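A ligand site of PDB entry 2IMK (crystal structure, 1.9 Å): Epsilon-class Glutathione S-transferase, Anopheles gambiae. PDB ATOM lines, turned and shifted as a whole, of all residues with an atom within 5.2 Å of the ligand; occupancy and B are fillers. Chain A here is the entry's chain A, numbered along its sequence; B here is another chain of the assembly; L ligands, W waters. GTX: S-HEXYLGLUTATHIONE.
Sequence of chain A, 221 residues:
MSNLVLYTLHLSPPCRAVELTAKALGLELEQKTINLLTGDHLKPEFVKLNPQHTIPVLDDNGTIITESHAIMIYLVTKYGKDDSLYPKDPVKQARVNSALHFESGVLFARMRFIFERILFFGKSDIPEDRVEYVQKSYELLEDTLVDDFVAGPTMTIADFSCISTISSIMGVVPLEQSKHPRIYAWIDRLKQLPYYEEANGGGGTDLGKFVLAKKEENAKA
The backbone carbonyl oxygen (O) of Ile 55 lies within hydrogen-bond range of a nitrogen (N2) of the ligand.
The side-chain carboxylate (OE1) of Glu 67 is in salt-bridge range of a nitrogen (N1) of the ligand, at 2.8 Å.
N of Ile 55 lies within hydrogen-bond range of O2 of the ligand (3.0 Å).
N of Ser 68 sits at hydrogen-bond distance from O12 of the ligand, at 2.9 Å.
The side-chain hydroxyl (OG) of Ser 12 lies close to a sulfur (SG2) of the ligand (3.4 Å).
NH1 of Arg 112 lies within salt-bridge range of O32 of the ligand (3.0 Å).
An oxygen (O31) of the ligand sits close to a ring nitrogen (NE2) of His 41 (3.5 Å).
An oxygen (O11) of the ligand sits at hydrogen-bond distance from the side-chain hydroxyl of Ser 68 (2.6 Å).
A ring nitrogen (ND1) of His 53 sits at hydrogen-bond distance from an oxygen (O31) of the ligand, at 3.2 Å.
N of Glu 67 sits at hydrogen-bond distance from O of Pro 56.
The backbone NH (N) of His 69 is in hydrogen-bond range of the side-chain carboxylate (OE2) of Glu 67, at 2.8 Å.
NE2 of His 69 sits close to OG of Ser 68, at 3.5 Å.
Merely in contact with the ligand: Leu 11, Pro 14, Leu 36, Thr 54, Pro 56, Phe 108, Leu 119 and Leu 207.
Hydrophobic or aromatic side chains that line the ligand: Leu 11, Pro 14, Leu 36, His 41, His 53, Ile 55, Pro 56, Phe 108, Leu 119 and Leu 207.
Within 4 Å of the ligand: Leu 11, Ser 12, Pro 14, Leu 36, His 41, His 53, Thr 54, Ile 55, Pro 56, Glu 67, Ser 68, Phe 108, Arg 112, Leu 119 and Leu 207.
The nearest printed residue that does not touch the ligand is Pro 13 (4.004 Å).
Water W2 lies within hydrogen-bond range of O12 of the ligand (2.6 Å), OG1 of Thr 54 (2.8 Å) and O of Pro 56 (2.8 Å).
Water W1 lies within hydrogen-bond range of an oxygen (OE1) of the ligand (2.7 Å) and the guanidinium group (NH1) of Arg 112 (3.2 Å).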
ATOM      1  N   LEU A   9      -2.943  11.859 -16.395  1.00  0.00           N
ATOM      2  CA  LEU A   9      -3.773  11.579 -17.553  1.00  0.00           C
ATOM      3  C   LEU A   9      -5.126  12.122 -17.134  1.00  0.00           C
ATOM      4  O   LEU A   9      -5.615  11.786 -16.096  1.00  0.00           O
ATOM      5  CB  LEU A   9      -3.835  10.077 -17.846  1.00  0.00           C
ATOM      6  CG  LEU A   9      -4.559   9.678 -19.139  1.00  0.00           C
ATOM      7  CD1 LEU A   9      -3.777  10.158 -20.430  1.00  0.00           C
ATOM      8  CD2 LEU A   9      -4.746   8.164 -19.115  1.00  0.00           C
ATOM      9  N   LEU A  11      -8.140  11.573 -17.941  1.00  0.00           N
ATOM     10  CA  LEU A  11      -9.203  10.616 -17.645  1.00  0.00           C
ATOM     11  C   LEU A  11      -9.161  10.002 -16.224  1.00  0.00           C
ATOM     12  O   LEU A  11     -10.156   9.542 -15.766  1.00  0.00           O
ATOM     13  CB  LEU A  11      -9.154   9.469 -18.657  1.00  0.00           C
ATOM     14  CG  LEU A  11      -9.439   9.839 -20.089  1.00  0.00           C
ATOM     15  CD1 LEU A  11      -9.734   8.530 -20.959  1.00  0.00           C
ATOM     16  CD2 LEU A  11     -10.595  10.804 -20.191  1.00  0.00           C
ATOM     17  N   SER A  12      -7.991   9.979 -15.618  1.00  0.00           N
ATOM     18  CA  SER A  12      -7.779   9.383 -14.283  1.00  0.00           C
ATOM     19  C   SER A  12      -8.425  10.227 -13.154  1.00  0.00           C
ATOM     20  O   SER A  12      -8.099  11.423 -13.017  1.00  0.00           O
ATOM     21  CB  SER A  12      -6.290   9.213 -14.036  1.00  0.00           C
ATOM     22  OG  SER A  12      -6.022   9.104 -12.624  1.00  0.00           O
ATOM     23  N   PRO A  13      -9.345   9.629 -12.373  1.00  0.00           N
ATOM     24  CA  PRO A  13      -9.960  10.402 -11.257  1.00  0.00           C
ATOM     25  C   PRO A  13      -8.966  10.999 -10.253  1.00  0.00           C
ATOM     26  O   PRO A  13      -9.065  12.202  -9.992  1.00  0.00           O
ATOM     27  CB  PRO A  13     -10.921   9.414 -10.613  1.00  0.00           C
ATOM     28  CG  PRO A  13     -11.134   8.356 -11.680  1.00  0.00           C
ATOM     29  CD  PRO A  13      -9.865   8.256 -12.435  1.00  0.00           C
ATOM     30  N   PRO A  14      -8.049  10.209  -9.686  1.00  0.00           N
ATOM     31  CA  PRO A  14      -7.128  10.864  -8.777  1.00  0.00           C
ATOM     32  C   PRO A  14      -6.294  12.013  -9.363  1.00  0.00           C
ATOM     33  O   PRO A  14      -5.968  12.922  -8.617  1.00  0.00           O
ATOM     34  CB  PRO A  14      -6.250   9.710  -8.252  1.00  0.00           C
ATOM     35  CG  PRO A  14      -6.430   8.607  -9.235  1.00  0.00           C
ATOM     36  CD  PRO A  14      -7.806   8.748  -9.680  1.00  0.00           C
ATOM     37  N   LEU A  36      -1.293   5.456 -19.772  1.00  0.00           N
ATOM     38  CA  LEU A  36      -1.524   4.150 -19.232  1.00  0.00           C
ATOM     39  C   LEU A  36      -1.956   3.169 -20.363  1.00  0.00           C
ATOM     40  O   LEU A  36      -1.707   1.959 -20.291  1.00  0.00           O
ATOM     41  CB  LEU A  36      -2.642   4.263 -18.211  1.00  0.00           C
ATOM     42  CG  LEU A  36      -2.451   5.132 -16.950  1.00  0.00           C
ATOM     43  CD1 LEU A  36      -3.756   5.095 -16.088  1.00  0.00           C
ATOM     44  CD2 LEU A  36      -1.269   4.670 -16.125  1.00  0.00           C
ATOM     45  N   LEU A  37      -2.630   3.684 -21.372  1.00  0.00           N
ATOM     46  CA  LEU A  37      -3.151   2.783 -22.402  1.00  0.00           C
ATOM     47  C   LEU A  37      -2.046   2.178 -23.286  1.00  0.00           C
ATOM     48  O   LEU A  37      -2.253   1.126 -23.924  1.00  0.00           O
ATOM     49  CB  LEU A  37      -4.191   3.499 -23.266  1.00  0.00           C
ATOM     50  CG  LEU A  37      -5.549   3.668 -22.618  1.00  0.00           C
ATOM     51  CD1 LEU A  37      -6.448   4.342 -23.660  1.00  0.00           C
ATOM     52  CD2 LEU A  37      -6.109   2.280 -22.191  1.00  0.00           C
ATOM     53  N   HIS A  41       3.329   4.037 -17.804  1.00  0.00           N
ATOM     54  CA  HIS A  41       3.571   3.802 -16.370  1.00  0.00           C
ATOM     55  C   HIS A  41       4.404   2.580 -16.013  1.00  0.00           C
ATOM     56  O   HIS A  41       4.976   2.471 -14.903  1.00  0.00           O
ATOM     57  CB  HIS A  41       2.232   3.727 -15.639  1.00  0.00           C
ATOM     58  CG  HIS A  41       1.376   2.548 -16.051  1.00  0.00           C
ATOM     59  ND1 HIS A  41       0.816   2.423 -17.310  1.00  0.00           N
ATOM     60  CD2 HIS A  41       0.938   1.486 -15.348  1.00  0.00           C
ATOM     61  CE1 HIS A  41       0.061   1.351 -17.356  1.00  0.00           C
ATOM     62  NE2 HIS A  41       0.137   0.741 -16.184  1.00  0.00           N
ATOM     63  N   LEU A  42       4.494   1.646 -16.962  1.00  0.00           N
ATOM     64  CA  LEU A  42       5.301   0.457 -16.751  1.00  0.00           C
ATOM     65  C   LEU A  42       6.753   0.637 -17.169  1.00  0.00           C
ATOM     66  O   LEU A  42       7.574  -0.252 -16.958  1.00  0.00           O
ATOM     67  CB  LEU A  42       4.687  -0.732 -17.476  1.00  0.00           C
ATOM     68  CG  LEU A  42       3.242  -0.981 -17.071  1.00  0.00           C
ATOM     69  CD1 LEU A  42       2.793  -2.208 -17.751  1.00  0.00           C
ATOM     70  CD2 LEU A  42       3.102  -1.119 -15.523  1.00  0.00           C
ATOM     71  N   GLN A  52       5.106   1.864  -7.095  1.00  0.00           N
ATOM     72  CA  GLN A  52       3.750   1.296  -7.290  1.00  0.00           C
ATOM     73  C   GLN A  52       3.251   1.606  -8.708  1.00  0.00           C
ATOM     74  O   GLN A  52       2.194   1.125  -9.127  1.00  0.00           O
ATOM     75  CB  GLN A  52       2.751   1.745  -6.189  1.00  0.00           C
ATOM     76  CG  GLN A  52       3.176   1.322  -4.777  1.00  0.00           C
ATOM     77  CD  GLN A  52       2.555   2.172  -3.616  1.00  0.00           C
ATOM     78  OE1 GLN A  52       2.898   1.952  -2.440  1.00  0.00           O
ATOM     79  NE2 GLN A  52       1.669   3.127  -3.934  1.00  0.00           N
ATOM     80  N   HIS A  53       4.057   2.319  -9.488  1.00  0.00           N
ATOM     81  CA  HIS A  53       3.684   2.723 -10.868  1.00  0.00           C
ATOM     82  C   HIS A  53       2.220   3.179 -11.068  1.00  0.00           C
ATOM     83  O   HIS A  53       1.557   2.740 -12.017  1.00  0.00           O
ATOM     84  CB  HIS A  53       4.111   1.688 -11.926  1.00  0.00           C
ATOM     85  CG  HIS A  53       3.605   0.303 -11.667  1.00  0.00           C
ATOM     86  ND1 HIS A  53       2.371  -0.129 -12.106  1.00  0.00           N
ATOM     87  CD2 HIS A  53       4.191  -0.758 -11.056  1.00  0.00           C
ATOM     88  CE1 HIS A  53       2.206  -1.390 -11.735  1.00  0.00           C
ATOM     89  NE2 HIS A  53       3.298  -1.806 -11.128  1.00  0.00           N
ATOM     90  N   THR A  54       1.724   4.041 -10.166  1.00  0.00           N
ATOM     91  CA  THR A  54       0.440   4.710 -10.416  1.00  0.00           C
ATOM     92  C   THR A  54       0.617   6.187 -10.702  1.00  0.00           C
ATOM     93  O   THR A  54       1.611   6.801 -10.290  1.00  0.00           O
ATOM     94  CB  THR A  54      -0.554   4.513  -9.232  1.00  0.00           C
ATOM     95  OG1 THR A  54      -0.018   5.074  -7.993  1.00  0.00           O
ATOM     96  CG2 THR A  54      -0.968   2.971  -9.097  1.00  0.00           C
ATOM     97  N   ILE A  55      -0.383   6.787 -11.363  1.00  0.00           N
ATOM     98  CA  ILE A  55      -0.569   8.245 -11.413  1.00  0.00           C
ATOM     99  C   ILE A  55      -1.749   8.671 -10.457  1.00  0.00           C
ATOM    100  O   ILE A  55      -2.717   7.947 -10.318  1.00  0.00           O
ATOM    101  CB  ILE A  55      -0.784   8.728 -12.877  1.00  0.00           C
ATOM    102  CG1 ILE A  55      -1.997   8.021 -13.513  1.00  0.00           C
ATOM    103  CG2 ILE A  55       0.560   8.593 -13.736  1.00  0.00           C
ATOM    104  CD1 ILE A  55      -2.460   8.646 -14.846  1.00  0.00           C
ATOM    105  N   PRO A  56      -1.729   9.902  -9.868  1.00  0.00           N
ATOM    106  CA  PRO A  56      -0.766  10.997 -10.178  1.00  0.00           C
ATOM    107  C   PRO A  56       0.524  10.832  -9.404  1.00  0.00           C
ATOM    108  O   PRO A  56       0.543  10.100  -8.358  1.00  0.00           O
ATOM    109  CB  PRO A  56      -1.507  12.282  -9.748  1.00  0.00           C
ATOM    110  CG  PRO A  56      -2.472  11.817  -8.583  1.00  0.00           C
ATOM    111  CD  PRO A  56      -2.796  10.319  -8.927  1.00  0.00           C
ATOM    112  N   GLU A  67       0.744   9.811  -4.929  1.00  0.00           N
ATOM    113  CA  GLU A  67      -0.549   9.362  -4.350  1.00  0.00           C
ATOM    114  C   GLU A  67      -1.446  10.580  -4.187  1.00  0.00           C
ATOM    115  O   GLU A  67      -1.033  11.496  -3.488  1.00  0.00           O
ATOM    116  CB  GLU A  67      -0.366   8.545  -3.058  1.00  0.00           C
ATOM    117  CG  GLU A  67      -1.560   7.602  -2.732  1.00  0.00           C
ATOM    118  CD  GLU A  67      -2.826   8.322  -2.260  1.00  0.00           C
ATOM    119  OE1 GLU A  67      -3.928   7.801  -2.574  1.00  0.00           O
ATOM    120  OE2 GLU A  67      -2.728   9.405  -1.579  1.00  0.00           O
ATOM    121  N   SER A  68      -2.585  10.637  -4.878  1.00  0.00           N
ATOM    122  CA  SER A  68      -3.435  11.857  -4.956  1.00  0.00           C
ATOM    123  C   SER A  68      -3.729  12.556  -3.587  1.00  0.00           C
ATOM    124  O   SER A  68      -3.710  13.797  -3.504  1.00  0.00           O
ATOM    125  CB  SER A  68      -4.751  11.566  -5.687  1.00  0.00           C
ATOM    126  OG  SER A  68      -5.622  10.690  -4.935  1.00  0.00           O
ATOM    127  N   HIS A  69      -3.961  11.751  -2.539  1.00  0.00           N
ATOM    128  CA  HIS A  69      -4.454  12.295  -1.251  1.00  0.00           C
ATOM    129  C   HIS A  69      -3.276  12.934  -0.539  1.00  0.00           C
ATOM    130  O   HIS A  69      -3.391  14.057  -0.081  1.00  0.00           O
ATOM    131  CB  HIS A  69      -5.163  11.239  -0.377  1.00  0.00           C
ATOM    132  CG  HIS A  69      -6.220  10.479  -1.121  1.00  0.00           C
ATOM    133  ND1 HIS A  69      -7.557  10.826  -1.106  1.00  0.00           N
ATOM    134  CD2 HIS A  69      -6.117   9.397  -1.936  1.00  0.00           C
ATOM    135  CE1 HIS A  69      -8.238   9.991  -1.869  1.00  0.00           C
ATOM    136  NE2 HIS A  69      -7.392   9.124  -2.395  1.00  0.00           N
ATOM    137  N   SER A 104     -10.400   6.519  -1.055  1.00  0.00           N
ATOM    138  CA  SER A 104      -9.438   5.512  -1.523  1.00  0.00           C
ATOM    139  C   SER A 104      -9.922   4.035  -1.282  1.00  0.00           C
ATOM    140  O   SER A 104      -9.840   3.207  -2.200  1.00  0.00           O
ATOM    141  CB  SER A 104      -8.022   5.815  -0.977  1.00  0.00           C
ATOM    142  OG  SER A 104      -7.937   5.544   0.412  1.00  0.00           O
ATOM    143  N   PHE A 108     -13.039   4.784  -4.852  1.00  0.00           N
ATOM    144  CA  PHE A 108     -12.075   4.423  -5.854  1.00  0.00           C
ATOM    145  C   PHE A 108     -11.785   2.927  -5.989  1.00  0.00           C
ATOM    146  O   PHE A 108     -11.709   2.444  -7.116  1.00  0.00           O
ATOM    147  CB  PHE A 108     -10.763   5.227  -5.717  1.00  0.00           C
ATOM    148  CG  PHE A 108      -9.803   5.028  -6.877  1.00  0.00           C
ATOM    149  CD1 PHE A 108      -8.747   4.139  -6.785  1.00  0.00           C
ATOM    150  CD2 PHE A 108      -9.974   5.731  -8.076  1.00  0.00           C
ATOM    151  CE1 PHE A 108      -7.881   3.949  -7.850  1.00  0.00           C
ATOM    152  CE2 PHE A 108      -9.151   5.557  -9.145  1.00  0.00           C
ATOM    153  CZ  PHE A 108      -8.097   4.714  -9.062  1.00  0.00           C
ATOM    154  N   MET A 111     -14.668   1.265  -7.906  1.00  0.00           N
ATOM    155  CA  MET A 111     -14.686   1.763  -9.287  1.00  0.00           C
ATOM    156  C   MET A 111     -13.594   1.100 -10.174  1.00  0.00           C
ATOM    157  O   MET A 111     -13.901   0.644 -11.274  1.00  0.00           O
ATOM    158  CB  MET A 111     -14.556   3.288  -9.353  1.00  0.00           C
ATOM    159  CG  MET A 111     -14.460   3.825 -10.771  1.00  0.00           C
ATOM    160  SD  MET A 111     -13.485   5.304 -10.954  1.00  0.00           S
ATOM    161  CE  MET A 111     -11.910   4.652 -11.531  1.00  0.00           C
ATOM    162  N   ARG A 112     -12.348   1.087  -9.681  1.00  0.00           N
ATOM    163  CA  ARG A 112     -11.234   0.298 -10.251  1.00  0.00           C
ATOM    164  C   ARG A 112     -11.429  -1.231 -10.379  1.00  0.00           C
ATOM    165  O   ARG A 112     -11.023  -1.824 -11.375  1.00  0.00           O
ATOM    166  CB  ARG A 112      -9.894   0.673  -9.583  1.00  0.00           C
ATOM    167  CG  ARG A 112      -8.750  -0.251 -10.030  1.00  0.00           C
ATOM    168  CD  ARG A 112      -7.382   0.371  -9.820  1.00  0.00           C
ATOM    169  NE  ARG A 112      -6.381  -0.615 -10.244  1.00  0.00           N
ATOM    170  CZ  ARG A 112      -5.062  -0.443 -10.255  1.00  0.00           C
ATOM    171  NH1 ARG A 112      -4.523   0.720  -9.849  1.00  0.00           N
ATOM    172  NH2 ARG A 112      -4.293  -1.459 -10.665  1.00  0.00           N
ATOM    173  N   LEU A 119     -10.655  -1.967 -19.219  1.00  0.00           N
ATOM    174  CA  LEU A 119      -9.711  -1.153 -19.922  1.00  0.00           C
ATOM    175  C   LEU A 119      -8.437  -1.928 -20.270  1.00  0.00           C
ATOM    176  O   LEU A 119      -7.871  -1.704 -21.317  1.00  0.00           O
ATOM    177  CB  LEU A 119      -9.379   0.106 -19.095  1.00  0.00           C
ATOM    178  CG  LEU A 119     -10.548   1.033 -18.840  1.00  0.00           C
ATOM    179  CD1 LEU A 119     -10.125   2.191 -17.938  1.00  0.00           C
ATOM    180  CD2 LEU A 119     -11.087   1.574 -20.133  1.00  0.00           C
ATOM    181  N   LEU A 207     -14.197   9.554 -19.147  1.00  0.00           N
ATOM    182  CA  LEU A 207     -13.802   8.236 -18.661  1.00  0.00           C
ATOM    183  C   LEU A 207     -14.981   7.253 -18.655  1.00  0.00           C
ATOM    184  O   LEU A 207     -14.809   6.079 -19.075  1.00  0.00           O
ATOM    185  CB  LEU A 207     -13.217   8.262 -17.237  1.00  0.00           C
ATOM    186  CG  LEU A 207     -12.739   6.849 -16.776  1.00  0.00           C
ATOM    187  CD1 LEU A 207     -11.659   6.237 -17.693  1.00  0.00           C
ATOM    188  CD2 LEU A 207     -12.218   6.890 -15.306  1.00  0.00           C
ATOM    189  N   PHE A 210     -15.631   6.234 -22.227  1.00  0.00           N
ATOM    190  CA  PHE A 210     -14.558   5.483 -22.810  1.00  0.00           C
ATOM    191  C   PHE A 210     -14.709   4.044 -22.291  1.00  0.00           C
ATOM    192  O   PHE A 210     -14.551   3.094 -23.059  1.00  0.00           O
ATOM    193  CB  PHE A 210     -13.194   6.127 -22.468  1.00  0.00           C
ATOM    194  CG  PHE A 210     -12.021   5.348 -23.004  1.00  0.00           C
ATOM    195  CD1 PHE A 210     -11.221   4.604 -22.154  1.00  0.00           C
ATOM    196  CD2 PHE A 210     -11.766   5.289 -24.385  1.00  0.00           C
ATOM    197  CE1 PHE A 210     -10.155   3.816 -22.651  1.00  0.00           C
ATOM    198  CE2 PHE A 210     -10.710   4.537 -24.879  1.00  0.00           C
ATOM    199  CZ  PHE A 210      -9.904   3.811 -23.987  1.00  0.00           C
ATOM    200  N   HIS B 101      -2.887   5.464   2.297  1.00  0.00           N
ATOM    201  CA  HIS B 101      -3.768   5.233   1.190  1.00  0.00           C
ATOM    202  C   HIS B 101      -3.478   3.958   0.345  1.00  0.00           C
ATOM    203  O   HIS B 101      -4.387   3.321  -0.196  1.00  0.00           O
ATOM    204  CB  HIS B 101      -3.868   6.526   0.349  1.00  0.00           C
ATOM    205  CG  HIS B 101      -4.619   7.592   1.054  1.00  0.00           C
ATOM    206  ND1 HIS B 101      -5.992   7.567   1.151  1.00  0.00           N
ATOM    207  CD2 HIS B 101      -4.205   8.624   1.831  1.00  0.00           C
ATOM    208  CE1 HIS B 101      -6.395   8.581   1.909  1.00  0.00           C
ATOM    209  NE2 HIS B 101      -5.329   9.230   2.326  1.00  0.00           N
HETATM  210  N1  GTX L   1      -4.564   5.817  -4.387  1.00  0.00           N
HETATM  211  CA1 GTX L   1      -4.107   6.151  -5.736  1.00  0.00           C
HETATM  212  C1  GTX L   1      -4.122   7.636  -5.899  1.00  0.00           C
HETATM  213  O11 GTX L   1      -5.170   8.259  -5.663  1.00  0.00           O
HETATM  214  O12 GTX L   1      -3.069   8.181  -6.250  1.00  0.00           O
HETATM  215  CB1 GTX L   1      -4.938   5.592  -6.909  1.00  0.00           C
HETATM  216  CG1 GTX L   1      -3.975   5.643  -8.100  1.00  0.00           C
HETATM  217  CD1 GTX L   1      -4.300   4.725  -9.246  1.00  0.00           C
HETATM  218  OE1 GTX L   1      -4.651   3.601  -8.988  1.00  0.00           O
HETATM  219  N2  GTX L   1      -4.236   5.245 -10.515  1.00  0.00           N
HETATM  220  CA2 GTX L   1      -4.484   4.423 -11.742  1.00  0.00           C
HETATM  221  C2  GTX L   1      -3.143   3.870 -12.245  1.00  0.00           C
HETATM  222  O2  GTX L   1      -2.144   4.581 -12.327  1.00  0.00           O
HETATM  223  CB2 GTX L   1      -5.051   5.437 -12.728  1.00  0.00           C
HETATM  224  SG2 GTX L   1      -6.714   5.784 -12.242  1.00  0.00           S
HETATM  225  C1S GTX L   1      -7.674   4.405 -12.789  1.00  0.00           C
HETATM  226  C2S GTX L   1      -8.393   4.900 -14.048  1.00  0.00           C
HETATM  227  C3S GTX L   1      -7.495   5.174 -15.264  1.00  0.00           C
HETATM  228  C4S GTX L   1      -8.294   5.088 -16.555  1.00  0.00           C
HETATM  229  C5S GTX L   1      -7.847   6.077 -17.625  1.00  0.00           C
HETATM  230  C6S GTX L   1      -7.867   5.504 -19.076  1.00  0.00           C
HETATM  231  N3  GTX L   1      -3.047   2.559 -12.530  1.00  0.00           N
HETATM  232  CA3 GTX L   1      -1.854   1.898 -12.979  1.00  0.00           C
HETATM  233  C3  GTX L   1      -1.472   0.593 -12.290  1.00  0.00           C
HETATM  234  O31 GTX L   1      -0.726  -0.157 -12.939  1.00  0.00           O
HETATM  235  O32 GTX L   1      -1.822   0.242 -11.134  1.00  0.00           O
HETATM  236  O   HOH W   1      -4.454   1.873  -6.879  1.00  0.00           O
HETATM  237  O   HOH W   2      -0.743   7.732  -7.434  1.00  0.00           O
HETATM  238  O   HOH W   3      -2.331   3.666  -3.845  1.00  0.00           O
HETATM  239  O   HOH W   4      -6.177   1.335 -13.331  1.00  0.00           O
HETATM  240  O   HOH W   5      -8.292   7.296  -5.592  1.00  0.00           O
